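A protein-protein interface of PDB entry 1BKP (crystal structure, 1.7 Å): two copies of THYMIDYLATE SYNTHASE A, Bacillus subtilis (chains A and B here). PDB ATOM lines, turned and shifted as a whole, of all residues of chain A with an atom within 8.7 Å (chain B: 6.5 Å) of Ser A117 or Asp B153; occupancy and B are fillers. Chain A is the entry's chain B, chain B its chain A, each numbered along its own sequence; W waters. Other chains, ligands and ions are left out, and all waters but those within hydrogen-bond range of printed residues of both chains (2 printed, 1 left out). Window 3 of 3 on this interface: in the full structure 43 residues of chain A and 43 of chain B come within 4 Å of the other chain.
The side-chain carboxylate (OD1) of Asp B153 is in salt-bridge range of the guanidinium group (NH2) of Arg A116, at 3.2 Å.
The side-chain amide oxygen (OD1) of Asn A115 lies close to the side-chain carboxylate (OD1) of Asp B150 (2.9 Å).
N of Ser A117 sits at hydrogen-bond distance from OD2 of Asp B153 (2.9 Å).
The side-chain carboxylate (OD2) of Asp B150 lies within salt-bridge range of the side-chain amino group (NZ) of Lys A113 (2.8 Å).
O of Lys A113 lies within hydrogen-bond range of ND2 of Asn A115 (3.4 Å).
O of Arg A116 is in hydrogen-bond range of N of Val A123, at 2.7 Å.
The backbone NH of Asp B150 lies within hydrogen-bond range of the side-chain amide oxygen of Asn B148 (3.0 Å).
The backbone NH (N) of Asn A115 is in hydrogen-bond range of the backbone carbonyl oxygen (O) of Val A123.
Among the printed residues, pairs that only touch across the chains: Asn A115 with Pro B149 (3.5 Å), Asn A115 with Asp B153 (3.6 Å) and Arg A116 with Leu B152 (3.3 Å).
Of the printed residues of chain B, Lys A113 touches Asp B150 (2.8 Å).
Printed residues of chain B within 4 Å of Asn A115: Pro B149 (3.5 Å), Asp B150 (2.9 Å) and Asp B153 (3.6 Å).
Of the printed residues of chain B, Arg A116 touches Leu B152 (3.3 Å) and Asp B153 (3.2 Å).
Ser A117 touches just one residue of chain B: Asp B153.
Asn A119 touches none of the printed residues of chain B.
Printed residues of chain A within 4 Å of Pro B149: Asn A115 (3.5 Å).
Of the printed residues of chain A, Leu B152 touches Arg A116.
Of chain A, only Asn A115 (3.6 Å), Arg A116 (3.2 Å) and Ser A117 (2.9 Å) come within 4 Å of Asp B153.
No residue of chain A comes within 4 Å of Ala B154.
Met B155 touches none of the printed residues of chain A.
The nearest printed residue of chain B that does not touch Ser A117 is Leu B152 (7.8 Å).
Of the 16 printed residues of chain A, 4 touch a printed residue of chain B.
Hydrophobic or aromatic side chains of chain B that line the printed part of chain A: Leu B152.
Among the printed residues, 7 pairs touch across the chains.
Among the printed residues, Asp or Glu carboxylates within 4 Å of a Lys or Arg side-chain nitrogen of the other chain: Lys A113 with Asp B150 (2.8 Å) and Arg A116 with Asp B153 (3.2 Å).
No position is printed for both chains.
Of the 7 pairs that touch across the chains among the printed residues, none has its exchanged pair printed and touching as well.
Water W1 lies within hydrogen-bond range of ND2 of Asn A115 and O of Pro B149.
Water W2 lies within hydrogen-bond range of the backbone carbonyl oxygen of Ser A117 and the side-chain carboxylate of Asp B153.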
ATOM      1  N   LYS A 113       7.989 -12.057  16.656  1.00  0.00           N
ATOM      2  CA  LYS A 113       7.409 -11.960  17.992  1.00  0.00           C
ATOM      3  C   LYS A 113       5.944 -12.247  17.929  1.00  0.00           C
ATOM      4  O   LYS A 113       5.259 -11.611  17.142  1.00  0.00           O
ATOM      5  CB  LYS A 113       7.549 -10.581  18.612  1.00  0.00           C
ATOM      6  CG  LYS A 113       8.939 -10.245  19.149  1.00  0.00           C
ATOM      7  CD  LYS A 113       9.031  -8.768  19.727  1.00  0.00           C
ATOM      8  CE  LYS A 113       8.547  -8.723  21.192  1.00  0.00           C
ATOM      9  NZ  LYS A 113       8.851  -7.336  21.703  1.00  0.00           N
ATOM     10  N   LYS A 114       5.434 -13.006  18.901  1.00  0.00           N
ATOM     11  CA  LYS A 114       4.030 -13.398  18.875  1.00  0.00           C
ATOM     12  C   LYS A 114       3.376 -12.388  19.704  1.00  0.00           C
ATOM     13  O   LYS A 114       3.332 -12.533  20.888  1.00  0.00           O
ATOM     14  CB  LYS A 114       3.828 -14.831  19.438  1.00  0.00           C
ATOM     15  CG  LYS A 114       4.599 -15.818  18.544  1.00  0.00           C
ATOM     16  CD  LYS A 114       4.312 -17.233  18.774  1.00  0.00           C
ATOM     17  CE  LYS A 114       5.180 -18.046  17.814  1.00  0.00           C
ATOM     18  NZ  LYS A 114       5.491 -17.340  16.471  1.00  0.00           N
ATOM     19  N   ASN A 115       2.888 -11.344  19.079  1.00  0.00           N
ATOM     20  CA  ASN A 115       2.337 -10.241  19.805  1.00  0.00           C
ATOM     21  C   ASN A 115       0.980  -9.829  19.302  1.00  0.00           C
ATOM     22  O   ASN A 115       0.499  -8.760  19.691  1.00  0.00           O
ATOM     23  CB  ASN A 115       3.307  -9.022  19.793  1.00  0.00           C
ATOM     24  CG  ASN A 115       3.786  -8.619  18.367  1.00  0.00           C
ATOM     25  OD1 ASN A 115       4.852  -7.953  18.196  1.00  0.00           O
ATOM     26  ND2 ASN A 115       3.037  -9.059  17.352  1.00  0.00           N
ATOM     27  N   ARG A 116       0.370 -10.622  18.415  1.00  0.00           N
ATOM     28  CA  ARG A 116      -0.966 -10.236  17.934  1.00  0.00           C
ATOM     29  C   ARG A 116      -1.983 -11.335  18.240  1.00  0.00           C
ATOM     30  O   ARG A 116      -1.765 -12.494  17.915  1.00  0.00           O
ATOM     31  CB  ARG A 116      -1.064 -10.002  16.416  1.00  0.00           C
ATOM     32  CG  ARG A 116      -0.251  -8.907  15.781  1.00  0.00           C
ATOM     33  CD  ARG A 116      -0.580  -7.563  16.360  1.00  0.00           C
ATOM     34  NE  ARG A 116      -1.996  -7.203  16.367  1.00  0.00           N
ATOM     35  CZ  ARG A 116      -2.614  -6.540  15.389  1.00  0.00           C
ATOM     36  NH1 ARG A 116      -1.939  -6.195  14.274  1.00  0.00           N
ATOM     37  NH2 ARG A 116      -3.790  -5.994  15.625  1.00  0.00           N
ATOM     38  N   SER A 117      -3.147 -10.931  18.699  1.00  0.00           N
ATOM     39  CA  SER A 117      -4.209 -11.887  18.986  1.00  0.00           C
ATOM     40  C   SER A 117      -4.993 -12.207  17.739  1.00  0.00           C
ATOM     41  O   SER A 117      -5.413 -11.297  17.019  1.00  0.00           O
ATOM     42  CB  SER A 117      -5.152 -11.309  20.016  1.00  0.00           C
ATOM     43  OG  SER A 117      -5.730 -12.425  20.683  1.00  0.00           O
ATOM     44  N   LEU A 118      -5.192 -13.490  17.475  1.00  0.00           N
ATOM     45  CA  LEU A 118      -5.915 -13.942  16.323  1.00  0.00           C
ATOM     46  C   LEU A 118      -6.552 -15.311  16.652  1.00  0.00           C
ATOM     47  O   LEU A 118      -5.848 -16.292  16.896  1.00  0.00           O
ATOM     48  CB  LEU A 118      -4.954 -14.118  15.158  1.00  0.00           C
ATOM     49  CG  LEU A 118      -5.705 -14.513  13.915  1.00  0.00           C
ATOM     50  CD1 LEU A 118      -6.519 -13.345  13.468  1.00  0.00           C
ATOM     51  CD2 LEU A 118      -4.750 -14.919  12.851  1.00  0.00           C
ATOM     52  N   ASN A 119      -7.880 -15.377  16.620  1.00  0.00           N
ATOM     53  CA  ASN A 119      -8.564 -16.638  16.902  1.00  0.00           C
ATOM     54  C   ASN A 119      -8.158 -17.150  18.264  1.00  0.00           C
ATOM     55  O   ASN A 119      -7.759 -18.293  18.393  1.00  0.00           O
ATOM     56  CB  ASN A 119      -8.220 -17.707  15.849  1.00  0.00           C
ATOM     57  CG  ASN A 119      -8.758 -17.367  14.489  1.00  0.00           C
ATOM     58  OD1 ASN A 119      -8.220 -17.806  13.472  1.00  0.00           O
ATOM     59  ND2 ASN A 119      -9.842 -16.598  14.456  1.00  0.00           N
ATOM     60  N   GLY A 120      -8.104 -16.253  19.238  1.00  0.00           N
ATOM     61  CA  GLY A 120      -7.757 -16.685  20.574  1.00  0.00           C
ATOM     62  C   GLY A 120      -6.354 -17.227  20.739  1.00  0.00           C
ATOM     63  O   GLY A 120      -6.071 -17.812  21.782  1.00  0.00           O
ATOM     64  N   GLU A 121      -5.483 -16.998  19.744  1.00  0.00           N
ATOM     65  CA  GLU A 121      -4.078 -17.433  19.768  1.00  0.00           C
ATOM     66  C   GLU A 121      -3.178 -16.191  19.508  1.00  0.00           C
ATOM     67  O   GLU A 121      -3.647 -15.263  18.931  1.00  0.00           O
ATOM     68  CB  GLU A 121      -3.910 -18.521  18.692  1.00  0.00           C
ATOM     69  CG  GLU A 121      -2.538 -19.097  18.455  1.00  0.00           C
ATOM     70  CD  GLU A 121      -2.463 -19.808  17.095  1.00  0.00           C
ATOM     71  OE1 GLU A 121      -3.529 -19.993  16.461  1.00  0.00           O
ATOM     72  OE2 GLU A 121      -1.350 -20.166  16.639  1.00  0.00           O
ATOM     73  N   LYS A 122      -1.914 -16.199  19.949  1.00  0.00           N
ATOM     74  CA  LYS A 122      -0.937 -15.116  19.790  1.00  0.00           C
ATOM     75  C   LYS A 122      -0.101 -15.473  18.581  1.00  0.00           C
ATOM     76  O   LYS A 122       0.416 -16.595  18.482  1.00  0.00           O
ATOM     77  CB  LYS A 122      -0.002 -15.020  20.993  1.00  0.00           C
ATOM     78  CG  LYS A 122      -0.556 -14.276  22.189  1.00  0.00           C
ATOM     79  CD  LYS A 122      -0.837 -12.803  21.909  1.00  0.00           C
ATOM     80  CE  LYS A 122      -1.235 -12.035  23.176  1.00  0.00           C
ATOM     81  NZ  LYS A 122      -1.553 -10.573  22.903  1.00  0.00           N
ATOM     82  N   VAL A 123      -0.072 -14.587  17.589  1.00  0.00           N
ATOM     83  CA  VAL A 123       0.652 -14.882  16.366  1.00  0.00           C
ATOM     84  C   VAL A 123       1.582 -13.694  16.029  1.00  0.00           C
ATOM     85  O   VAL A 123       1.427 -12.577  16.596  1.00  0.00           O
ATOM     86  CB  VAL A 123      -0.330 -15.175  15.167  1.00  0.00           C
ATOM     87  CG1 VAL A 123      -1.229 -16.452  15.426  1.00  0.00           C
ATOM     88  CG2 VAL A 123      -1.132 -13.943  14.730  1.00  0.00           C
ATOM     89  N   ASP A 124       2.543 -13.951  15.147  1.00  0.00           N
ATOM     90  CA  ASP A 124       3.507 -12.884  14.774  1.00  0.00           C
ATOM     91  C   ASP A 124       2.944 -11.995  13.625  1.00  0.00           C
ATOM     92  O   ASP A 124       1.833 -12.211  13.071  1.00  0.00           O
ATOM     93  CB  ASP A 124       4.910 -13.443  14.450  1.00  0.00           C
ATOM     94  CG  ASP A 124       4.915 -14.381  13.255  1.00  0.00           C
ATOM     95  OD1 ASP A 124       4.243 -14.100  12.235  1.00  0.00           O
ATOM     96  OD2 ASP A 124       5.615 -15.404  13.333  1.00  0.00           O
ATOM     97  N   TYR A 128      -0.099 -13.004  10.932  1.00  0.00           N
ATOM     98  CA  TYR A 128      -1.216 -12.151  11.035  1.00  0.00           C
ATOM     99  C   TYR A 128      -1.540 -11.530   9.694  1.00  0.00           C
ATOM    100  O   TYR A 128      -2.684 -11.480   9.286  1.00  0.00           O
ATOM    101  CB  TYR A 128      -0.947 -11.039  12.064  1.00  0.00           C
ATOM    102  CG  TYR A 128      -2.238 -10.208  12.371  1.00  0.00           C
ATOM    103  CD1 TYR A 128      -3.190 -10.646  13.308  1.00  0.00           C
ATOM    104  CD2 TYR A 128      -2.485  -9.032  11.730  1.00  0.00           C
ATOM    105  CE1 TYR A 128      -4.379  -9.908  13.584  1.00  0.00           C
ATOM    106  CE2 TYR A 128      -3.679  -8.245  12.004  1.00  0.00           C
ATOM    107  CZ  TYR A 128      -4.595  -8.711  12.916  1.00  0.00           C
ATOM    108  OH  TYR A 128      -5.736  -7.973  13.113  1.00  0.00           O
ATOM    109  N   HIS A 131      -3.033 -14.125   7.217  1.00  0.00           N
ATOM    110  CA  HIS A 131      -4.411 -14.409   7.518  1.00  0.00           C
ATOM    111  C   HIS A 131      -5.313 -13.240   7.053  1.00  0.00           C
ATOM    112  O   HIS A 131      -6.390 -13.458   6.443  1.00  0.00           O
ATOM    113  CB  HIS A 131      -4.586 -14.566   9.034  1.00  0.00           C
ATOM    114  CG  HIS A 131      -6.017 -14.809   9.441  1.00  0.00           C
ATOM    115  ND1 HIS A 131      -6.574 -16.080   9.491  1.00  0.00           N
ATOM    116  CD2 HIS A 131      -7.029 -13.947   9.717  1.00  0.00           C
ATOM    117  CE1 HIS A 131      -7.863 -15.989   9.774  1.00  0.00           C
ATOM    118  NE2 HIS A 131      -8.164 -14.713   9.909  1.00  0.00           N
ATOM    119  N   GLN A 132      -4.946 -12.006   7.472  1.00  0.00           N
ATOM    120  CA  GLN A 132      -5.736 -10.826   7.144  1.00  0.00           C
ATOM    121  C   GLN A 132      -5.821 -10.511   5.623  1.00  0.00           C
ATOM    122  O   GLN A 132      -6.880 -10.025   5.085  1.00  0.00           O
ATOM    123  CB  GLN A 132      -5.150  -9.645   7.932  1.00  0.00           C
ATOM    124  CG  GLN A 132      -5.435  -9.679   9.449  1.00  0.00           C
ATOM    125  CD  GLN A 132      -6.947  -9.629   9.788  1.00  0.00           C
ATOM    126  OE1 GLN A 132      -7.558 -10.680  10.058  1.00  0.00           O
ATOM    127  NE2 GLN A 132      -7.554  -8.430   9.706  1.00  0.00           N
ATOM    128  N   ARG A 141      -5.246  -1.380   7.277  1.00  0.00           N
ATOM    129  CA  ARG A 141      -4.170  -1.603   8.248  1.00  0.00           C
ATOM    130  C   ARG A 141      -3.215  -2.785   8.012  1.00  0.00           C
ATOM    131  O   ARG A 141      -2.728  -3.360   9.015  1.00  0.00           O
ATOM    132  CB  ARG A 141      -4.750  -1.879   9.639  1.00  0.00           C
ATOM    133  CG  ARG A 141      -5.721  -0.887  10.095  1.00  0.00           C
ATOM    134  CD  ARG A 141      -6.295  -1.376  11.393  1.00  0.00           C
ATOM    135  NE  ARG A 141      -7.610  -0.808  11.550  1.00  0.00           N
ATOM    136  CZ  ARG A 141      -8.582  -1.342  12.273  1.00  0.00           C
ATOM    137  NH1 ARG A 141      -8.373  -2.463  12.952  1.00  0.00           N
ATOM    138  NH2 ARG A 141      -9.757  -0.718  12.334  1.00  0.00           N
ATOM    139  N   ASN B 148       3.347   0.843  17.174  1.00  0.00           N
ATOM    140  CA  ASN B 148       4.158  -0.031  17.989  1.00  0.00           C
ATOM    141  C   ASN B 148       3.498  -1.423  17.821  1.00  0.00           C
ATOM    142  O   ASN B 148       2.438  -1.681  18.388  1.00  0.00           O
ATOM    143  CB  ASN B 148       4.042   0.388  19.456  1.00  0.00           C
ATOM    144  CG  ASN B 148       4.924  -0.469  20.378  1.00  0.00           C
ATOM    145  OD1 ASN B 148       5.167  -1.661  20.109  1.00  0.00           O
ATOM    146  ND2 ASN B 148       5.308   0.097  21.529  1.00  0.00           N
ATOM    147  N   PRO B 149       4.205  -2.358  17.147  1.00  0.00           N
ATOM    148  CA  PRO B 149       3.668  -3.719  16.888  1.00  0.00           C
ATOM    149  C   PRO B 149       3.303  -4.565  18.117  1.00  0.00           C
ATOM    150  O   PRO B 149       2.420  -5.390  18.047  1.00  0.00           O
ATOM    151  CB  PRO B 149       4.752  -4.372  15.989  1.00  0.00           C
ATOM    152  CG  PRO B 149       6.048  -3.587  16.375  1.00  0.00           C
ATOM    153  CD  PRO B 149       5.620  -2.205  16.721  1.00  0.00           C
ATOM    154  N   ASP B 150       3.942  -4.274  19.231  1.00  0.00           N
ATOM    155  CA  ASP B 150       3.729  -5.046  20.459  1.00  0.00           C
ATOM    156  C   ASP B 150       2.465  -4.605  21.174  1.00  0.00           C
ATOM    157  O   ASP B 150       1.968  -5.317  22.026  1.00  0.00           O
ATOM    158  CB  ASP B 150       4.885  -4.789  21.437  1.00  0.00           C
ATOM    159  CG  ASP B 150       6.128  -5.570  21.108  1.00  0.00           C
ATOM    160  OD1 ASP B 150       6.071  -6.644  20.526  1.00  0.00           O
ATOM    161  OD2 ASP B 150       7.193  -5.132  21.487  1.00  0.00           O
ATOM    162  N   GLU B 151       1.947  -3.450  20.806  1.00  0.00           N
ATOM    163  CA  GLU B 151       0.819  -2.923  21.544  1.00  0.00           C
ATOM    164  C   GLU B 151      -0.419  -2.584  20.745  1.00  0.00           C
ATOM    165  O   GLU B 151      -1.386  -2.067  21.334  1.00  0.00           O
ATOM    166  CB  GLU B 151       1.278  -1.657  22.335  1.00  0.00           C
ATOM    167  CG  GLU B 151       2.382  -1.985  23.313  1.00  0.00           C
ATOM    168  CD  GLU B 151       2.378  -1.014  24.530  1.00  0.00           C
ATOM    169  OE1 GLU B 151       2.870   0.101  24.472  1.00  0.00           O
ATOM    170  OE2 GLU B 151       1.820  -1.411  25.552  1.00  0.00           O
ATOM    171  N   LEU B 152      -0.494  -3.044  19.503  1.00  0.00           N
ATOM    172  CA  LEU B 152      -1.674  -2.724  18.674  1.00  0.00           C
ATOM    173  C   LEU B 152      -2.997  -3.202  19.324  1.00  0.00           C
ATOM    174  O   LEU B 152      -3.994  -2.474  19.352  1.00  0.00           O
ATOM    175  CB  LEU B 152      -1.549  -3.327  17.264  1.00  0.00           C
ATOM    176  CG  LEU B 152      -0.375  -2.742  16.466  1.00  0.00           C
ATOM    177  CD1 LEU B 152      -0.080  -3.553  15.148  1.00  0.00           C
ATOM    178  CD2 LEU B 152      -0.665  -1.228  16.226  1.00  0.00           C
ATOM    179  N   ASP B 153      -2.928  -4.334  19.999  1.00  0.00           N
ATOM    180  CA  ASP B 153      -4.147  -4.887  20.574  1.00  0.00           C
ATOM    181  C   ASP B 153      -4.583  -4.139  21.800  1.00  0.00           C
ATOM    182  O   ASP B 153      -5.692  -4.297  22.236  1.00  0.00           O
ATOM    183  CB  ASP B 153      -3.989  -6.377  20.890  1.00  0.00           C
ATOM    184  CG  ASP B 153      -3.859  -7.220  19.650  1.00  0.00           C
ATOM    185  OD1 ASP B 153      -4.536  -6.912  18.620  1.00  0.00           O
ATOM    186  OD2 ASP B 153      -3.066  -8.154  19.686  1.00  0.00           O
ATOM    187  N   ALA B 154      -3.690  -3.356  22.363  1.00  0.00           N
ATOM    188  CA  ALA B 154      -4.015  -2.571  23.540  1.00  0.00           C
ATOM    189  C   ALA B 154      -4.454  -1.151  23.186  1.00  0.00           C
ATOM    190  O   ALA B 154      -4.561  -0.259  24.061  1.00  0.00           O
ATOM    191  CB  ALA B 154      -2.818  -2.550  24.447  1.00  0.00           C
ATOM    192  N   MET B 155      -4.640  -0.902  21.883  1.00  0.00           N
ATOM    193  CA  MET B 155      -5.032   0.436  21.466  1.00  0.00           C
ATOM    194  C   MET B 155      -6.531   0.461  21.120  1.00  0.00           C
ATOM    195  O   MET B 155      -7.018  -0.440  20.431  1.00  0.00           O
ATOM    196  CB  MET B 155      -4.245   0.864  20.243  1.00  0.00           C
ATOM    197  CG  MET B 155      -2.738   0.760  20.398  1.00  0.00           C
ATOM    198  SD  MET B 155      -1.929   1.462  18.888  1.00  0.00           S
ATOM    199  CE  MET B 155      -0.256   1.108  19.399  1.00  0.00           C
ATOM    200  N   ALA B 156      -7.253   1.471  21.620  1.00  0.00           N
ATOM    201  CA  ALA B 156      -8.706   1.595  21.330  1.00  0.00           C
ATOM    202  C   ALA B 156      -8.907   1.897  19.853  1.00  0.00           C
ATOM    203  O   ALA B 156      -9.973   1.616  19.297  1.00  0.00           O
ATOM    204  CB  ALA B 156      -9.343   2.711  22.179  1.00  0.00           C
HETATM  205  O   HOH W   1       2.465  -6.984  15.599  1.00  0.00           O
HETATM  206  O   HOH W   2      -6.127  -8.540  16.618  1.00  0.00           O
